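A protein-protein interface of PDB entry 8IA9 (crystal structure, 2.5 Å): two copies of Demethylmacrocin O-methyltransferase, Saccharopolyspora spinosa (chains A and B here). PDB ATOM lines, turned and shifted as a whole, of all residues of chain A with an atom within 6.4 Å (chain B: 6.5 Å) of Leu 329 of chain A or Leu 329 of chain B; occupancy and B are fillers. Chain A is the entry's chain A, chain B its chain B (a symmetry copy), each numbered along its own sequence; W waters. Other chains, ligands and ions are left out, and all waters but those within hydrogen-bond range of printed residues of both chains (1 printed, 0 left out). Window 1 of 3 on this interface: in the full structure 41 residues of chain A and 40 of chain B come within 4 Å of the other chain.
NZ of Lys 326 of chain A lies within salt-bridge range of OE1 of Glu 330 of chain B, at 2.6 Å.
The side-chain amino group of Lys 326 of chain B is in salt-bridge range of the side-chain carboxylate of Glu 330 of chain A (2.9 Å).
The side-chain amide nitrogen (NE2) of Gln 333 of chain A lies within hydrogen-bond range of the backbone carbonyl oxygen (O) of Tyr 358 of chain B, at 3.2 Å.
The backbone carbonyl oxygen (O) of Leu 355 of chain A lies within hydrogen-bond range of the backbone NH (N) of Thr 357 of chain B (3.0 Å).
The backbone carbonyl oxygen (O) of Thr 357 of chain A is in hydrogen-bond range of the backbone NH (N) of Leu 355 of chain B (2.8 Å).
O of Tyr 358 of chain A is in hydrogen-bond range of NE2 of Gln 333 of chain B (2.9 Å).
Leu 300 of chain A touches Gln 333 of chain B (CD1 to NE2, 3.97 Å).
O of Leu 325 of chain A touches CD1 of Leu 329 of chain B, 3.96 Å away.
Leu 329 of chain B touches Leu 329 of chain A (CD1 to CD1, 3.8 Å).
Thr 357 of chain B touches Leu 329 of chain A (OG1 to CD1, 3.4 Å).
Glu 330 of chain A touches Val 322 of chain B.
Gln 333 of chain A touches Leu 300 of chain B.
CG2 of Thr 357 of chain B touches NE2 of Gln 333 of chain A (3.6 Å).
O of Leu 355 of chain B touches O of Leu 355 of chain A (3.6 Å).
Leu 329 of chain B touches Thr 357 of chain A (CD1 to OG1, 3.3 Å).
Tyr 358 of chain A touches Val 332 of chain B.
Leu 329 of chain A touches just these residues of chain B: Leu 325 (3.9 Å), Leu 329 (3.8 Å) and Thr 357 (3.4 Å).
Leu 329 of chain B touches just these residues of chain A: Leu 325 (3.96 Å), Leu 329 (3.8 Å) and Thr 357 (3.3 Å).
Of the printed residues of chain B, Lys 326 of chain A touches Lys 326 and Glu 330.
Of the printed residues of chain B, Thr 357 of chain A touches Leu 329, Gln 333 and Leu 355.
Printed residues of chain B within 4 Å of Glu 330 of chain A: Val 322 (3.8 Å) and Lys 326 (2.9 Å).
Of the printed residues of chain B, Val 332 of chain A touches Tyr 358.
Leu 324 of chain A touches none of the printed residues of chain B.
The nearest residue of chain B that does not touch Leu 329 of chain A is Leu 355 of chain B (4.1 Å).
Hydrophobic or aromatic side chains of chain B within 4 Å of the printed part of chain A: Leu 300, Val 322, Leu 329 and Val 332.
Among the printed residues, 21 pairs touch across the chains.
Leu 325 of chain A touches Leu 329 of chain B, and with the chains exchanged Leu 329 of chain A touches Leu 325 of chain B.
Lys 326 of chain A touches its own counterpart, Lys 326 of chain B.
Leu 329 of chain A touches Thr 357 of chain B, and with the chains exchanged Thr 357 of chain A touches Leu 329 of chain B.
Gln 333 of chain A touches Thr 357 of chain B, and with the chains exchanged Thr 357 of chain A touches Gln 333 of chain B.
17 positions are printed for both chains.
Water W1 lies within hydrogen-bond range of the backbone carbonyl oxygen (O) of Leu 355 of chain A (2.8 Å), the backbone carbonyl oxygen (O) of Leu 355 of chain B (2.9 Å), the side-chain hydroxyl (OG1) of Thr 357 of chain A (3.0 Å) and the side-chain hydroxyl (OG1) of Thr 357 of chain B (3.3 Å).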
ATOM      1  N   LEU A 300      -9.122 -36.308 -21.807  1.00  0.00           N
ATOM      2  CA  LEU A 300      -7.698 -36.000 -22.110  1.00  0.00           C
ATOM      3  C   LEU A 300      -6.779 -36.589 -21.023  1.00  0.00           C
ATOM      4  O   LEU A 300      -5.561 -36.694 -21.256  1.00  0.00           O
ATOM      5  CB  LEU A 300      -7.533 -34.480 -22.202  1.00  0.00           C
ATOM      6  CG  LEU A 300      -8.492 -33.762 -23.152  1.00  0.00           C
ATOM      7  CD1 LEU A 300      -8.160 -32.284 -23.243  1.00  0.00           C
ATOM      8  CD2 LEU A 300      -8.482 -34.372 -24.544  1.00  0.00           C
ATOM      9  N   VAL A 322      -2.246 -34.659 -24.750  1.00  0.00           N
ATOM     10  CA  VAL A 322      -2.013 -33.236 -24.355  1.00  0.00           C
ATOM     11  C   VAL A 322      -0.852 -32.663 -25.171  1.00  0.00           C
ATOM     12  O   VAL A 322      -0.960 -31.518 -25.624  1.00  0.00           O
ATOM     13  CB  VAL A 322      -1.810 -33.054 -22.838  1.00  0.00           C
ATOM     14  CG1 VAL A 322      -1.247 -31.680 -22.497  1.00  0.00           C
ATOM     15  CG2 VAL A 322      -3.107 -33.285 -22.079  1.00  0.00           C
ATOM     16  N   LEU A 324      -0.115 -33.621 -28.215  1.00  0.00           N
ATOM     17  CA  LEU A 324      -0.759 -33.491 -29.550  1.00  0.00           C
ATOM     18  C   LEU A 324      -1.500 -32.146 -29.615  1.00  0.00           C
ATOM     19  O   LEU A 324      -1.147 -31.332 -30.484  1.00  0.00           O
ATOM     20  CB  LEU A 324      -1.690 -34.691 -29.767  1.00  0.00           C
ATOM     21  CG  LEU A 324      -2.669 -34.590 -30.941  1.00  0.00           C
ATOM     22  CD1 LEU A 324      -1.936 -34.460 -32.263  1.00  0.00           C
ATOM     23  CD2 LEU A 324      -3.597 -35.792 -30.983  1.00  0.00           C
ATOM     24  N   LEU A 325      -2.272 -31.824 -28.575  1.00  0.00           N
ATOM     25  CA  LEU A 325      -3.073 -30.573 -28.506  1.00  0.00           C
ATOM     26  C   LEU A 325      -2.129 -29.362 -28.476  1.00  0.00           C
ATOM     27  O   LEU A 325      -2.451 -28.351 -29.130  1.00  0.00           O
ATOM     28  CB  LEU A 325      -3.980 -30.619 -27.271  1.00  0.00           C
ATOM     29  CG  LEU A 325      -5.097 -31.665 -27.305  1.00  0.00           C
ATOM     30  CD1 LEU A 325      -5.924 -31.635 -26.025  1.00  0.00           C
ATOM     31  CD2 LEU A 325      -6.006 -31.454 -28.501  1.00  0.00           C
ATOM     32  N   LYS A 326      -0.958 -29.489 -27.836  1.00  0.00           N
ATOM     33  CA  LYS A 326       0.048 -28.398 -27.747  1.00  0.00           C
ATOM     34  C   LYS A 326       0.600 -28.134 -29.149  1.00  0.00           C
ATOM     35  O   LYS A 326       0.587 -26.960 -29.565  1.00  0.00           O
ATOM     36  CB  LYS A 326       1.170 -28.736 -26.757  1.00  0.00           C
ATOM     37  CG  LYS A 326       0.751 -28.751 -25.294  1.00  0.00           C
ATOM     38  CD  LYS A 326       1.727 -29.433 -24.354  1.00  0.00           C
ATOM     39  CE  LYS A 326       2.786 -28.516 -23.790  1.00  0.00           C
ATOM     40  NZ  LYS A 326       3.524 -29.177 -22.687  1.00  0.00           N
ATOM     41  N   ASN A 327       0.854 -29.198 -29.918  1.00  0.00           N
ATOM     42  CA  ASN A 327       1.469 -29.106 -31.269  1.00  0.00           C
ATOM     43  C   ASN A 327       0.445 -28.538 -32.262  1.00  0.00           C
ATOM     44  O   ASN A 327       0.808 -27.594 -33.002  1.00  0.00           O
ATOM     45  CB  ASN A 327       2.074 -30.446 -31.687  1.00  0.00           C
ATOM     46  CG  ASN A 327       3.281 -30.810 -30.842  1.00  0.00           C
ATOM     47  OD1 ASN A 327       4.009 -29.936 -30.371  1.00  0.00           O
ATOM     48  ND2 ASN A 327       3.442 -32.090 -30.555  1.00  0.00           N
ATOM     49  N   LEU A 328      -0.819 -28.963 -32.156  1.00  0.00           N
ATOM     50  CA  LEU A 328      -1.962 -28.396 -32.919  1.00  0.00           C
ATOM     51  C   LEU A 328      -2.035 -26.880 -32.692  1.00  0.00           C
ATOM     52  O   LEU A 328      -2.272 -26.151 -33.683  1.00  0.00           O
ATOM     53  CB  LEU A 328      -3.260 -29.074 -32.472  1.00  0.00           C
ATOM     54  CG  LEU A 328      -3.486 -30.494 -32.991  1.00  0.00           C
ATOM     55  CD1 LEU A 328      -4.930 -30.904 -32.763  1.00  0.00           C
ATOM     56  CD2 LEU A 328      -3.138 -30.608 -34.466  1.00  0.00           C
ATOM     57  N   LEU A 329      -1.883 -26.437 -31.435  1.00  0.00           N
ATOM     58  CA  LEU A 329      -1.967 -25.002 -31.040  1.00  0.00           C
ATOM     59  C   LEU A 329      -0.865 -24.221 -31.761  1.00  0.00           C
ATOM     60  O   LEU A 329      -1.204 -23.276 -32.494  1.00  0.00           O
ATOM     61  CB  LEU A 329      -1.841 -24.871 -29.519  1.00  0.00           C
ATOM     62  CG  LEU A 329      -2.057 -23.467 -28.952  1.00  0.00           C
ATOM     63  CD1 LEU A 329      -2.430 -23.523 -27.476  1.00  0.00           C
ATOM     64  CD2 LEU A 329      -0.828 -22.597 -29.145  1.00  0.00           C
ATOM     65  N   GLU A 330       0.351 -24.767 -31.783  1.00  0.00           N
ATOM     66  CA  GLU A 330       1.492 -24.167 -32.523  1.00  0.00           C
ATOM     67  C   GLU A 330       1.240 -24.294 -34.034  1.00  0.00           C
ATOM     68  O   GLU A 330       1.498 -23.323 -34.763  1.00  0.00           O
ATOM     69  CB  GLU A 330       2.815 -24.806 -32.106  1.00  0.00           C
ATOM     70  CG  GLU A 330       4.011 -24.022 -32.603  1.00  0.00           C
ATOM     71  CD  GLU A 330       5.220 -24.013 -31.684  1.00  0.00           C
ATOM     72  OE1 GLU A 330       5.413 -24.981 -30.917  1.00  0.00           O
ATOM     73  OE2 GLU A 330       5.978 -23.031 -31.746  1.00  0.00           O
ATOM     74  N   GLY A 331       0.532 -25.340 -34.444  1.00  0.00           N
ATOM     75  CA  GLY A 331       0.224 -25.590 -35.865  1.00  0.00           C
ATOM     76  C   GLY A 331      -0.645 -24.494 -36.462  1.00  0.00           C
ATOM     77  O   GLY A 331      -0.477 -24.173 -37.654  1.00  0.00           O
ATOM     78  N   VAL A 332      -1.498 -23.872 -35.652  1.00  0.00           N
ATOM     79  CA  VAL A 332      -2.458 -22.849 -36.143  1.00  0.00           C
ATOM     80  C   VAL A 332      -1.674 -21.591 -36.524  1.00  0.00           C
ATOM     81  O   VAL A 332      -2.054 -20.955 -37.516  1.00  0.00           O
ATOM     82  CB  VAL A 332      -3.542 -22.575 -35.089  1.00  0.00           C
ATOM     83  CG1 VAL A 332      -4.383 -21.364 -35.438  1.00  0.00           C
ATOM     84  CG2 VAL A 332      -4.414 -23.794 -34.861  1.00  0.00           C
ATOM     85  N   GLN A 333      -0.492 -21.400 -35.934  1.00  0.00           N
ATOM     86  CA  GLN A 333       0.386 -20.231 -36.209  1.00  0.00           C
ATOM     87  C   GLN A 333       1.395 -20.546 -37.326  1.00  0.00           C
ATOM     88  O   GLN A 333       2.336 -19.759 -37.497  1.00  0.00           O
ATOM     89  CB  GLN A 333       1.161 -19.855 -34.949  1.00  0.00           C
ATOM     90  CG  GLN A 333       0.358 -20.007 -33.670  1.00  0.00           C
ATOM     91  CD  GLN A 333      -0.951 -19.263 -33.732  1.00  0.00           C
ATOM     92  OE1 GLN A 333      -1.031 -18.172 -34.289  1.00  0.00           O
ATOM     93  NE2 GLN A 333      -1.976 -19.845 -33.125  1.00  0.00           N
ATOM     94  N   HIS A 334       1.193 -21.625 -38.084  1.00  0.00           N
ATOM     95  CA  HIS A 334       2.237 -22.204 -38.976  1.00  0.00           C
ATOM     96  C   HIS A 334       2.786 -21.130 -39.915  1.00  0.00           C
ATOM     97  O   HIS A 334       3.997 -21.140 -40.163  1.00  0.00           O
ATOM     98  CB  HIS A 334       1.712 -23.411 -39.764  1.00  0.00           C
ATOM     99  CG  HIS A 334       0.714 -23.048 -40.807  1.00  0.00           C
ATOM    100  ND1 HIS A 334      -0.651 -23.078 -40.564  1.00  0.00           N
ATOM    101  CD2 HIS A 334       0.866 -22.740 -42.116  1.00  0.00           C
ATOM    102  CE1 HIS A 334      -1.298 -22.832 -41.686  1.00  0.00           C
ATOM    103  NE2 HIS A 334      -0.390 -22.610 -42.650  1.00  0.00           N
ATOM    104  N   LEU A 352      -6.926 -26.752 -39.510  1.00  0.00           N
ATOM    105  CA  LEU A 352      -7.353 -26.484 -38.114  1.00  0.00           C
ATOM    106  C   LEU A 352      -7.319 -24.968 -37.874  1.00  0.00           C
ATOM    107  O   LEU A 352      -6.235 -24.384 -38.000  1.00  0.00           O
ATOM    108  CB  LEU A 352      -6.455 -27.241 -37.133  1.00  0.00           C
ATOM    109  CG  LEU A 352      -6.830 -27.062 -35.663  1.00  0.00           C
ATOM    110  CD1 LEU A 352      -8.168 -27.742 -35.349  1.00  0.00           C
ATOM    111  CD2 LEU A 352      -5.736 -27.577 -34.752  1.00  0.00           C
ATOM    112  N   LEU A 355      -8.924 -24.098 -31.998  1.00  0.00           N
ATOM    113  CA  LEU A 355      -8.718 -25.169 -30.994  1.00  0.00           C
ATOM    114  C   LEU A 355      -9.204 -24.665 -29.634  1.00  0.00           C
ATOM    115  O   LEU A 355      -8.765 -23.592 -29.207  1.00  0.00           O
ATOM    116  CB  LEU A 355      -7.240 -25.545 -30.948  1.00  0.00           C
ATOM    117  CG  LEU A 355      -6.832 -26.485 -29.818  1.00  0.00           C
ATOM    118  CD1 LEU A 355      -7.485 -27.843 -29.992  1.00  0.00           C
ATOM    119  CD2 LEU A 355      -5.318 -26.620 -29.745  1.00  0.00           C
ATOM    120  N   THR A 357      -9.713 -25.555 -25.738  1.00  0.00           N
ATOM    121  CA  THR A 357      -9.281 -26.451 -24.643  1.00  0.00           C
ATOM    122  C   THR A 357      -9.993 -26.101 -23.340  1.00  0.00           C
ATOM    123  O   THR A 357      -9.890 -24.921 -22.885  1.00  0.00           O
ATOM    124  CB  THR A 357      -7.772 -26.388 -24.439  1.00  0.00           C
ATOM    125  OG1 THR A 357      -7.179 -26.468 -25.736  1.00  0.00           O
ATOM    126  CG2 THR A 357      -7.298 -27.511 -23.541  1.00  0.00           C
ATOM    127  N   TYR A 358     -10.705 -27.085 -22.783  1.00  0.00           N
ATOM    128  CA  TYR A 358     -11.317 -27.025 -21.430  1.00  0.00           C
ATOM    129  C   TYR A 358     -10.829 -28.216 -20.602  1.00  0.00           C
ATOM    130  O   TYR A 358     -10.064 -29.032 -21.121  1.00  0.00           O
ATOM    131  CB  TYR A 358     -12.841 -27.027 -21.537  1.00  0.00           C
ATOM    132  CG  TYR A 358     -13.409 -26.057 -22.546  1.00  0.00           C
ATOM    133  CD1 TYR A 358     -13.687 -24.744 -22.213  1.00  0.00           C
ATOM    134  CD2 TYR A 358     -13.801 -26.495 -23.799  1.00  0.00           C
ATOM    135  CE1 TYR A 358     -14.201 -23.857 -23.151  1.00  0.00           C
ATOM    136  CE2 TYR A 358     -14.403 -25.648 -24.715  1.00  0.00           C
ATOM    137  CZ  TYR A 358     -14.570 -24.316 -24.404  1.00  0.00           C
ATOM    138  OH  TYR A 358     -15.214 -23.514 -25.294  1.00  0.00           O
ATOM    139  N   LEU B 300       0.199 -13.003 -31.743  1.00  0.00           N
ATOM    140  CA  LEU B 300       1.001 -14.150 -31.255  1.00  0.00           C
ATOM    141  C   LEU B 300       2.313 -14.272 -32.047  1.00  0.00           C
ATOM    142  O   LEU B 300       3.246 -14.943 -31.544  1.00  0.00           O
ATOM    143  CB  LEU B 300       0.170 -15.428 -31.413  1.00  0.00           C
ATOM    144  CG  LEU B 300      -1.174 -15.452 -30.689  1.00  0.00           C
ATOM    145  CD1 LEU B 300      -1.798 -16.838 -30.764  1.00  0.00           C
ATOM    146  CD2 LEU B 300      -1.020 -15.015 -29.236  1.00  0.00           C
ATOM    147  N   VAL B 322       3.650 -18.216 -27.572  1.00  0.00           N
ATOM    148  CA  VAL B 322       3.070 -19.528 -27.991  1.00  0.00           C
ATOM    149  C   VAL B 322       3.424 -20.606 -26.961  1.00  0.00           C
ATOM    150  O   VAL B 322       2.545 -21.444 -26.667  1.00  0.00           O
ATOM    151  CB  VAL B 322       3.473 -19.931 -29.418  1.00  0.00           C
ATOM    152  CG1 VAL B 322       3.197 -21.407 -29.673  1.00  0.00           C
ATOM    153  CG2 VAL B 322       2.757 -19.057 -30.444  1.00  0.00           C
ATOM    154  N   SER B 323       4.642 -20.580 -26.416  1.00  0.00           N
ATOM    155  CA  SER B 323       5.092 -21.514 -25.351  1.00  0.00           C
ATOM    156  C   SER B 323       4.183 -21.347 -24.125  1.00  0.00           C
ATOM    157  O   SER B 323       3.724 -22.361 -23.559  1.00  0.00           O
ATOM    158  CB  SER B 323       6.555 -21.278 -25.020  1.00  0.00           C
ATOM    159  OG  SER B 323       6.970 -22.091 -23.934  1.00  0.00           O
ATOM    160  N   LEU B 324       3.862 -20.098 -23.792  1.00  0.00           N
ATOM    161  CA  LEU B 324       2.978 -19.729 -22.662  1.00  0.00           C
ATOM    162  C   LEU B 324       1.595 -20.346 -22.904  1.00  0.00           C
ATOM    163  O   LEU B 324       1.139 -21.111 -22.037  1.00  0.00           O
ATOM    164  CB  LEU B 324       2.934 -18.201 -22.601  1.00  0.00           C
ATOM    165  CG  LEU B 324       2.016 -17.590 -21.550  1.00  0.00           C
ATOM    166  CD1 LEU B 324       2.535 -17.848 -20.143  1.00  0.00           C
ATOM    167  CD2 LEU B 324       1.864 -16.093 -21.780  1.00  0.00           C
ATOM    168  N   LEU B 325       1.078 -20.244 -24.134  1.00  0.00           N
ATOM    169  CA  LEU B 325      -0.285 -20.730 -24.472  1.00  0.00           C
ATOM    170  C   LEU B 325      -0.324 -22.260 -24.371  1.00  0.00           C
ATOM    171  O   LEU B 325      -1.334 -22.790 -23.849  1.00  0.00           O
ATOM    172  CB  LEU B 325      -0.682 -20.232 -25.863  1.00  0.00           C
ATOM    173  CG  LEU B 325      -0.898 -18.723 -25.988  1.00  0.00           C
ATOM    174  CD1 LEU B 325      -1.211 -18.342 -27.431  1.00  0.00           C
ATOM    175  CD2 LEU B 325      -2.010 -18.246 -25.057  1.00  0.00           C
ATOM    176  N   LYS B 326       0.802 -22.918 -24.657  1.00  0.00           N
ATOM    177  CA  LYS B 326       0.957 -24.396 -24.562  1.00  0.00           C
ATOM    178  C   LYS B 326       0.957 -24.831 -23.086  1.00  0.00           C
ATOM    179  O   LYS B 326       0.296 -25.845 -22.770  1.00  0.00           O
ATOM    180  CB  LYS B 326       2.221 -24.824 -25.310  1.00  0.00           C
ATOM    181  CG  LYS B 326       2.158 -24.633 -26.821  1.00  0.00           C
ATOM    182  CD  LYS B 326       3.485 -24.837 -27.541  1.00  0.00           C
ATOM    183  CE  LYS B 326       3.890 -26.290 -27.659  1.00  0.00           C
ATOM    184  NZ  LYS B 326       5.116 -26.465 -28.478  1.00  0.00           N
ATOM    185  N   ASN B 327       1.542 -24.022 -22.197  1.00  0.00           N
ATOM    186  CA  ASN B 327       1.607 -24.298 -20.731  1.00  0.00           C
ATOM    187  C   ASN B 327       0.244 -24.041 -20.077  1.00  0.00           C
ATOM    188  O   ASN B 327      -0.207 -24.917 -19.306  1.00  0.00           O
ATOM    189  CB  ASN B 327       2.743 -23.518 -20.067  1.00  0.00           C
ATOM    190  CG  ASN B 327       4.089 -24.099 -20.444  1.00  0.00           C
ATOM    191  OD1 ASN B 327       4.227 -25.317 -20.539  1.00  0.00           O
ATOM    192  ND2 ASN B 327       5.019 -23.249 -20.846  1.00  0.00           N
ATOM    193  N   LEU B 328      -0.440 -22.960 -20.467  1.00  0.00           N
ATOM    194  CA  LEU B 328      -1.830 -22.662 -20.015  1.00  0.00           C
ATOM    195  C   LEU B 328      -2.754 -23.826 -20.391  1.00  0.00           C
ATOM    196  O   LEU B 328      -3.585 -24.207 -19.537  1.00  0.00           O
ATOM    197  CB  LEU B 328      -2.316 -21.366 -20.666  1.00  0.00           C
ATOM    198  CG  LEU B 328      -1.655 -20.102 -20.140  1.00  0.00           C
ATOM    199  CD1 LEU B 328      -2.380 -18.877 -20.661  1.00  0.00           C
ATOM    200  CD2 LEU B 328      -1.633 -20.115 -18.619  1.00  0.00           C
ATOM    201  N   LEU B 329      -2.610 -24.349 -21.620  1.00  0.00           N
ATOM    202  CA  LEU B 329      -3.418 -25.473 -22.164  1.00  0.00           C
ATOM    203  C   LEU B 329      -3.207 -26.691 -21.263  1.00  0.00           C
ATOM    204  O   LEU B 329      -4.207 -27.234 -20.773  1.00  0.00           O
ATOM    205  CB  LEU B 329      -3.023 -25.767 -23.620  1.00  0.00           C
ATOM    206  CG  LEU B 329      -3.862 -26.838 -24.324  1.00  0.00           C
ATOM    207  CD1 LEU B 329      -3.851 -26.665 -25.832  1.00  0.00           C
ATOM    208  CD2 LEU B 329      -3.383 -28.231 -23.964  1.00  0.00           C
ATOM    209  N   GLU B 330      -1.961 -26.986 -20.902  1.00  0.00           N
ATOM    210  CA  GLU B 330      -1.635 -28.132 -20.018  1.00  0.00           C
ATOM    211  C   GLU B 330      -2.105 -27.798 -18.598  1.00  0.00           C
ATOM    212  O   GLU B 330      -2.678 -28.687 -17.938  1.00  0.00           O
ATOM    213  CB  GLU B 330      -0.144 -28.446 -20.105  1.00  0.00           C
ATOM    214  CG  GLU B 330       0.237 -29.688 -19.330  1.00  0.00           C
ATOM    215  CD  GLU B 330       1.402 -30.498 -19.874  1.00  0.00           C
ATOM    216  OE1 GLU B 330       2.273 -29.930 -20.587  1.00  0.00           O
ATOM    217  OE2 GLU B 330       1.420 -31.710 -19.589  1.00  0.00           O
ATOM    218  N   GLY B 331      -2.113 -26.510 -18.253  1.00  0.00           N
ATOM    219  CA  GLY B 331      -2.531 -26.032 -16.921  1.00  0.00           C
ATOM    220  C   GLY B 331      -3.993 -26.334 -16.648  1.00  0.00           C
ATOM    221  O   GLY B 331      -4.332 -26.660 -15.489  1.00  0.00           O
ATOM    222  N   VAL B 332      -4.818 -26.360 -17.696  1.00  0.00           N
ATOM    223  CA  VAL B 332      -6.285 -26.586 -17.565  1.00  0.00           C
ATOM    224  C   VAL B 332      -6.519 -28.023 -17.090  1.00  0.00           C
ATOM    225  O   VAL B 332      -7.500 -28.254 -16.366  1.00  0.00           O
ATOM    226  CB  VAL B 332      -7.002 -26.265 -18.887  1.00  0.00           C
ATOM    227  CG1 VAL B 332      -8.464 -26.695 -18.869  1.00  0.00           C
ATOM    228  CG2 VAL B 332      -6.866 -24.790 -19.229  1.00  0.00           C
ATOM    229  N   GLN B 333      -5.571 -28.921 -17.364  1.00  0.00           N
ATOM    230  CA  GLN B 333      -5.668 -30.355 -16.983  1.00  0.00           C
ATOM    231  C   GLN B 333      -4.925 -30.620 -15.664  1.00  0.00           C
ATOM    232  O   GLN B 333      -4.799 -31.806 -15.307  1.00  0.00           O
ATOM    233  CB  GLN B 333      -5.088 -31.237 -18.092  1.00  0.00           C
ATOM    234  CG  GLN B 333      -5.499 -30.829 -19.503  1.00  0.00           C
ATOM    235  CD  GLN B 333      -6.988 -30.613 -19.681  1.00  0.00           C
ATOM    236  OE1 GLN B 333      -7.825 -31.352 -19.167  1.00  0.00           O
ATOM    237  NE2 GLN B 333      -7.330 -29.592 -20.450  1.00  0.00           N
ATOM    238  N   HIS B 334      -4.589 -29.580 -14.894  1.00  0.00           N
ATOM    239  CA  HIS B 334      -3.713 -29.695 -13.693  1.00  0.00           C
ATOM    240  C   HIS B 334      -4.196 -30.823 -12.771  1.00  0.00           C
ATOM    241  O   HIS B 334      -3.337 -31.523 -12.214  1.00  0.00           O
ATOM    242  CB  HIS B 334      -3.599 -28.366 -12.931  1.00  0.00           C
ATOM    243  CG  HIS B 334      -4.836 -27.961 -12.203  1.00  0.00           C
ATOM    244  ND1 HIS B 334      -5.793 -27.142 -12.779  1.00  0.00           N
ATOM    245  CD2 HIS B 334      -5.261 -28.214 -10.947  1.00  0.00           C
ATOM    246  CE1 HIS B 334      -6.758 -26.910 -11.910  1.00  0.00           C
ATOM    247  NE2 HIS B 334      -6.468 -27.578 -10.787  1.00  0.00           N
ATOM    248  N   LEU B 352      -8.247 -20.504 -14.978  1.00  0.00           N
ATOM    249  CA  LEU B 352      -8.408 -20.595 -16.451  1.00  0.00           C
ATOM    250  C   LEU B 352      -9.234 -21.848 -16.788  1.00  0.00           C
ATOM    251  O   LEU B 352      -8.741 -22.966 -16.565  1.00  0.00           O
ATOM    252  CB  LEU B 352      -7.024 -20.617 -17.099  1.00  0.00           C
ATOM    253  CG  LEU B 352      -7.016 -20.688 -18.623  1.00  0.00           C
ATOM    254  CD1 LEU B 352      -7.556 -19.403 -19.231  1.00  0.00           C
ATOM    255  CD2 LEU B 352      -5.620 -20.957 -19.139  1.00  0.00           C
ATOM    256  N   LEU B 355      -9.407 -22.134 -22.995  1.00  0.00           N
ATOM    257  CA  LEU B 355      -8.392 -21.470 -23.838  1.00  0.00           C
ATOM    258  C   LEU B 355      -8.786 -21.654 -25.299  1.00  0.00           C
ATOM    259  O   LEU B 355      -8.963 -22.799 -25.699  1.00  0.00           O
ATOM    260  CB  LEU B 355      -7.025 -22.095 -23.573  1.00  0.00           C
ATOM    261  CG  LEU B 355      -5.903 -21.508 -24.407  1.00  0.00           C
ATOM    262  CD1 LEU B 355      -5.746 -20.045 -24.062  1.00  0.00           C
ATOM    263  CD2 LEU B 355      -4.608 -22.273 -24.192  1.00  0.00           C
ATOM    264  N   THR B 357      -7.662 -20.846 -29.105  1.00  0.00           N
ATOM    265  CA  THR B 357      -6.478 -20.519 -29.939  1.00  0.00           C
ATOM    266  C   THR B 357      -6.861 -20.527 -31.416  1.00  0.00           C
ATOM    267  O   THR B 357      -7.386 -21.552 -31.898  1.00  0.00           O
ATOM    268  CB  THR B 357      -5.319 -21.480 -29.671  1.00  0.00           C
ATOM    269  OG1 THR B 357      -4.925 -21.322 -28.303  1.00  0.00           O
ATOM    270  CG2 THR B 357      -4.148 -21.211 -30.586  1.00  0.00           C
ATOM    271  N   TYR B 358      -6.781 -19.356 -32.035  1.00  0.00           N
ATOM    272  CA  TYR B 358      -6.989 -19.137 -33.484  1.00  0.00           C
ATOM    273  C   TYR B 358      -5.693 -18.586 -34.092  1.00  0.00           C
ATOM    274  O   TYR B 358      -4.739 -18.326 -33.334  1.00  0.00           O
ATOM    275  CB  TYR B 358      -8.156 -18.176 -33.695  1.00  0.00           C
ATOM    276  CG  TYR B 358      -9.411 -18.533 -32.936  1.00  0.00           C
ATOM    277  CD1 TYR B 358     -10.377 -19.340 -33.503  1.00  0.00           C
ATOM    278  CD2 TYR B 358      -9.721 -17.919 -31.728  1.00  0.00           C
ATOM    279  CE1 TYR B 358     -11.597 -19.561 -32.878  1.00  0.00           C
ATOM    280  CE2 TYR B 358     -10.909 -18.181 -31.062  1.00  0.00           C
ATOM    281  CZ  TYR B 358     -11.865 -18.993 -31.649  1.00  0.00           C
ATOM    282  OH  TYR B 358     -13.080 -19.203 -31.054  1.00  0.00           O
HETATM  283  O   HOH W   1      -6.737 -23.909 -27.264  1.00  0.00           O
